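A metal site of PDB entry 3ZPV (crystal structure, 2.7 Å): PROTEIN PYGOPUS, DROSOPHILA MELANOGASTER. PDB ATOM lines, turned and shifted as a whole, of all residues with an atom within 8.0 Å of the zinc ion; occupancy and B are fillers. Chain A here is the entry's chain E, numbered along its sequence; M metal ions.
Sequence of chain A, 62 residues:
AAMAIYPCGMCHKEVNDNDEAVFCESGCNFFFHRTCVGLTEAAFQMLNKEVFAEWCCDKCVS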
ATOM      1  N   PHE A  23      -2.870  -2.683   3.459  1.00  0.00           N
ATOM      2  CA  PHE A  23      -2.646  -2.317   4.838  1.00  0.00           C
ATOM      3  C   PHE A  23      -2.521  -0.836   4.940  1.00  0.00           C
ATOM      4  O   PHE A  23      -1.774  -0.220   4.204  1.00  0.00           O
ATOM      5  CB  PHE A  23      -1.359  -2.970   5.312  1.00  0.00           C
ATOM      6  CG  PHE A  23      -1.035  -2.669   6.735  1.00  0.00           C
ATOM      7  CD1 PHE A  23      -1.715  -3.319   7.753  1.00  0.00           C
ATOM      8  CD2 PHE A  23      -0.074  -1.760   7.052  1.00  0.00           C
ATOM      9  CE1 PHE A  23      -1.443  -3.032   9.078  1.00  0.00           C
ATOM     10  CE2 PHE A  23       0.212  -1.475   8.363  1.00  0.00           C
ATOM     11  CZ  PHE A  23      -0.476  -2.093   9.382  1.00  0.00           C
ATOM     12  N   CYS A  24      -3.254  -0.228   5.861  1.00  0.00           N
ATOM     13  CA  CYS A  24      -3.199   1.221   6.012  1.00  0.00           C
ATOM     14  C   CYS A  24      -1.981   1.557   6.853  1.00  0.00           C
ATOM     15  O   CYS A  24      -1.938   1.275   8.047  1.00  0.00           O
ATOM     16  CB  CYS A  24      -4.494   1.770   6.633  1.00  0.00           C
ATOM     17  SG  CYS A  24      -4.508   3.593   6.801  1.00  0.00           S
ATOM     18  N   GLU A  25      -1.019   2.211   6.239  1.00  0.00           N
ATOM     19  CA  GLU A  25       0.201   2.621   6.940  1.00  0.00           C
ATOM     20  C   GLU A  25       0.110   4.069   7.553  1.00  0.00           C
ATOM     21  O   GLU A  25       1.043   4.529   8.173  1.00  0.00           O
ATOM     22  CB  GLU A  25       1.451   2.413   6.026  1.00  0.00           C
ATOM     23  CG  GLU A  25       2.188   1.000   5.953  1.00  0.00           C
ATOM     24  CD  GLU A  25       3.192   0.582   7.018  1.00  0.00           C
ATOM     25  OE1 GLU A  25       3.199   1.141   8.135  1.00  0.00           O
ATOM     26  OE2 GLU A  25       3.934  -0.436   6.787  1.00  0.00           O
ATOM     27  N   SER A  26      -1.005   4.764   7.388  1.00  0.00           N
ATOM     28  CA  SER A  26      -1.125   6.155   7.846  1.00  0.00           C
ATOM     29  C   SER A  26      -1.698   6.301   9.243  1.00  0.00           C
ATOM     30  O   SER A  26      -1.989   7.414   9.648  1.00  0.00           O
ATOM     31  CB  SER A  26      -1.974   6.999   6.869  1.00  0.00           C
ATOM     32  OG  SER A  26      -1.309   7.145   5.629  1.00  0.00           O
ATOM     33  N   GLY A  27      -1.929   5.204   9.971  1.00  0.00           N
ATOM     34  CA  GLY A  27      -2.373   5.386  11.368  1.00  0.00           C
ATOM     35  C   GLY A  27      -3.289   4.367  11.999  1.00  0.00           C
ATOM     36  O   GLY A  27      -3.026   3.961  13.108  1.00  0.00           O
ATOM     37  N   CYS A  28      -4.347   3.953  11.311  1.00  0.00           N
ATOM     38  CA  CYS A  28      -5.284   2.987  11.924  1.00  0.00           C
ATOM     39  C   CYS A  28      -4.692   1.588  12.121  1.00  0.00           C
ATOM     40  O   CYS A  28      -5.149   0.837  12.952  1.00  0.00           O
ATOM     41  CB  CYS A  28      -6.608   2.924  11.149  1.00  0.00           C
ATOM     42  SG  CYS A  28      -6.576   2.231   9.490  1.00  0.00           S
ATOM     43  N   ASN A  29      -3.666   1.253  11.341  1.00  0.00           N
ATOM     44  CA  ASN A  29      -3.034  -0.064  11.420  1.00  0.00           C
ATOM     45  C   ASN A  29      -3.943  -1.268  11.173  1.00  0.00           C
ATOM     46  O   ASN A  29      -3.670  -2.350  11.642  1.00  0.00           O
ATOM     47  CB  ASN A  29      -2.339  -0.238  12.766  1.00  0.00           C
ATOM     48  CG  ASN A  29      -1.044   0.554  12.841  1.00  0.00           C
ATOM     49  OD1 ASN A  29      -0.550   1.082  11.847  1.00  0.00           O
ATOM     50  ND2 ASN A  29      -0.489   0.632  14.028  1.00  0.00           N
ATOM     51  N   PHE A  30      -4.968  -1.077  10.369  1.00  0.00           N
ATOM     52  CA  PHE A  30      -5.810  -2.152   9.938  1.00  0.00           C
ATOM     53  C   PHE A  30      -5.412  -2.734   8.566  1.00  0.00           C
ATOM     54  O   PHE A  30      -5.036  -1.994   7.664  1.00  0.00           O
ATOM     55  CB  PHE A  30      -7.256  -1.663   9.803  1.00  0.00           C
ATOM     56  CG  PHE A  30      -8.048  -1.768  11.063  1.00  0.00           C
ATOM     57  CD1 PHE A  30      -8.625  -2.978  11.437  1.00  0.00           C
ATOM     58  CD2 PHE A  30      -8.218  -0.649  11.876  1.00  0.00           C
ATOM     59  CE1 PHE A  30      -9.380  -3.071  12.601  1.00  0.00           C
ATOM     60  CE2 PHE A  30      -8.966  -0.743  13.033  1.00  0.00           C
ATOM     61  CZ  PHE A  30      -9.556  -1.963  13.395  1.00  0.00           C
ATOM     62  N   PHE A  32      -7.100  -4.552   5.278  1.00  0.00           N
ATOM     63  CA  PHE A  32      -8.399  -4.497   4.599  1.00  0.00           C
ATOM     64  C   PHE A  32      -8.408  -5.422   3.403  1.00  0.00           C
ATOM     65  O   PHE A  32      -7.396  -5.545   2.722  1.00  0.00           O
ATOM     66  CB  PHE A  32      -8.647  -3.109   4.036  1.00  0.00           C
ATOM     67  CG  PHE A  32      -8.727  -2.019   5.054  1.00  0.00           C
ATOM     68  CD1 PHE A  32      -7.594  -1.449   5.563  1.00  0.00           C
ATOM     69  CD2 PHE A  32      -9.977  -1.514   5.451  1.00  0.00           C
ATOM     70  CE1 PHE A  32      -7.684  -0.419   6.506  1.00  0.00           C
ATOM     71  CE2 PHE A  32     -10.077  -0.476   6.366  1.00  0.00           C
ATOM     72  CZ  PHE A  32      -8.938   0.073   6.900  1.00  0.00           C
ATOM     73  N   TRP A  55      -0.706   2.814   0.281  1.00  0.00           N
ATOM     74  CA  TRP A  55      -2.139   3.036   0.348  1.00  0.00           C
ATOM     75  C   TRP A  55      -2.584   3.575   1.705  1.00  0.00           C
ATOM     76  O   TRP A  55      -1.939   3.341   2.726  1.00  0.00           O
ATOM     77  CB  TRP A  55      -2.868   1.726   0.028  1.00  0.00           C
ATOM     78  CG  TRP A  55      -4.349   1.826   0.107  1.00  0.00           C
ATOM     79  CD1 TRP A  55      -5.175   2.316  -0.838  1.00  0.00           C
ATOM     80  CD2 TRP A  55      -5.168   1.412   1.206  1.00  0.00           C
ATOM     81  NE1 TRP A  55      -6.472   2.261  -0.393  1.00  0.00           N
ATOM     82  CE2 TRP A  55      -6.498   1.728   0.868  1.00  0.00           C
ATOM     83  CE3 TRP A  55      -4.917   0.825   2.447  1.00  0.00           C
ATOM     84  CZ2 TRP A  55      -7.568   1.436   1.695  1.00  0.00           C
ATOM     85  CZ3 TRP A  55      -5.973   0.564   3.285  1.00  0.00           C
ATOM     86  CH2 TRP A  55      -7.293   0.862   2.901  1.00  0.00           C
ATOM     87  N   CYS A  56      -3.718   4.264   1.712  1.00  0.00           N
ATOM     88  CA  CYS A  56      -4.313   4.871   2.914  1.00  0.00           C
ATOM     89  C   CYS A  56      -5.841   4.751   2.915  1.00  0.00           C
ATOM     90  O   CYS A  56      -6.479   4.957   1.876  1.00  0.00           O
ATOM     91  CB  CYS A  56      -3.917   6.338   2.941  1.00  0.00           C
ATOM     92  SG  CYS A  56      -4.499   7.244   4.391  1.00  0.00           S
ATOM     93  N   CYS A  57      -6.435   4.377   4.059  1.00  0.00           N
ATOM     94  CA  CYS A  57      -7.895   4.211   4.139  1.00  0.00           C
ATOM     95  C   CYS A  57      -8.556   5.574   4.155  1.00  0.00           C
ATOM     96  O   CYS A  57      -7.894   6.589   4.344  1.00  0.00           O
ATOM     97  CB  CYS A  57      -8.313   3.413   5.388  1.00  0.00           C
ATOM     98  SG  CYS A  57      -8.192   4.263   6.997  1.00  0.00           S
ATOM     99  N   ASP A  58      -9.871   5.610   3.963  1.00  0.00           N
ATOM    100  CA  ASP A  58     -10.601   6.882   3.874  1.00  0.00           C
ATOM    101  C   ASP A  58     -10.614   7.661   5.187  1.00  0.00           C
ATOM    102  O   ASP A  58     -10.464   8.887   5.164  1.00  0.00           O
ATOM    103  CB  ASP A  58     -12.022   6.680   3.354  1.00  0.00           C
ATOM    104  CG  ASP A  58     -12.065   6.356   1.854  1.00  0.00           C
ATOM    105  OD1 ASP A  58     -11.114   6.726   1.123  1.00  0.00           O
ATOM    106  OD2 ASP A  58     -13.032   5.723   1.399  1.00  0.00           O
ATOM    107  N   LYS A  59     -10.766   6.971   6.307  1.00  0.00           N
ATOM    108  CA  LYS A  59     -10.728   7.611   7.607  1.00  0.00           C
ATOM    109  C   LYS A  59      -9.414   8.292   7.925  1.00  0.00           C
ATOM    110  O   LYS A  59      -9.386   9.347   8.548  1.00  0.00           O
ATOM    111  CB  LYS A  59     -11.069   6.612   8.717  1.00  0.00           C
ATOM    112  CG  LYS A  59     -12.564   6.363   8.862  1.00  0.00           C
ATOM    113  CD  LYS A  59     -12.893   5.045   9.517  1.00  0.00           C
ATOM    114  CE  LYS A  59     -14.322   4.596   9.159  1.00  0.00           C
ATOM    115  NZ  LYS A  59     -14.698   3.269   9.722  1.00  0.00           N
ATOM    116  N   CYS A  60      -8.316   7.697   7.526  1.00  0.00           N
ATOM    117  CA  CYS A  60      -6.997   8.255   7.868  1.00  0.00           C
ATOM    118  C   CYS A  60      -6.567   9.397   6.965  1.00  0.00           C
ATOM    119  O   CYS A  60      -5.689  10.158   7.334  1.00  0.00           O
ATOM    120  CB  CYS A  60      -5.921   7.151   7.861  1.00  0.00           C
ATOM    121  SG  CYS A  60      -6.087   5.939   9.192  1.00  0.00           S
ATOM    122  N   VAL A  61      -7.169   9.525   5.784  1.00  0.00           N
ATOM    123  CA  VAL A  61      -6.829  10.616   4.851  1.00  0.00           C
ATOM    124  C   VAL A  61      -6.962  11.960   5.537  1.00  0.00           C
ATOM    125  O   VAL A  61      -6.039  12.804   5.486  1.00  0.00           O
ATOM    126  CB  VAL A  61      -7.739  10.621   3.594  1.00  0.00           C
ATOM    127  CG1 VAL A  61      -7.496  11.874   2.753  1.00  0.00           C
ATOM    128  CG2 VAL A  61      -7.490   9.370   2.767  1.00  0.00           C
HETATM  129 ZN    ZN M   1      -6.357   3.928   8.144  1.00  0.00          ZN
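Four residues have an atom within 4 Å of the zinc ion: Cys 24, Cys 28, Cys 57 and Cys 60. Along chain A the residues within 4 Å of the zinc ion span positions 24 to 60. The nearest printed residue that does not touch the zinc ion is Phe 32 (4.8 Å).
The backbone NH of Lys 59 sits close to the side-chain sulfur of Cys 57, at 3.8 Å. The backbone NH (N) of Cys 24 is in hydrogen-bond range of the backbone carbonyl oxygen (O) of Phe 30. The side-chain sulfur of Cys 28 lies close to the backbone NH of Phe 30, 3.8 Å away. The side-chain sulfur (SG) of Cys 24 sits close to the backbone NH (N) of Ser 26.
The zinc ion is bound by the side-chain sulfur (SG) of Cys 28 (2.2 Å), the side-chain sulfur (SG) of Cys 57 (2.2 Å), the side-chain sulfur (SG) of Cys 60 (2.3 Å) and the side-chain sulfur (SG) of Cys 24 (2.3 Å).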
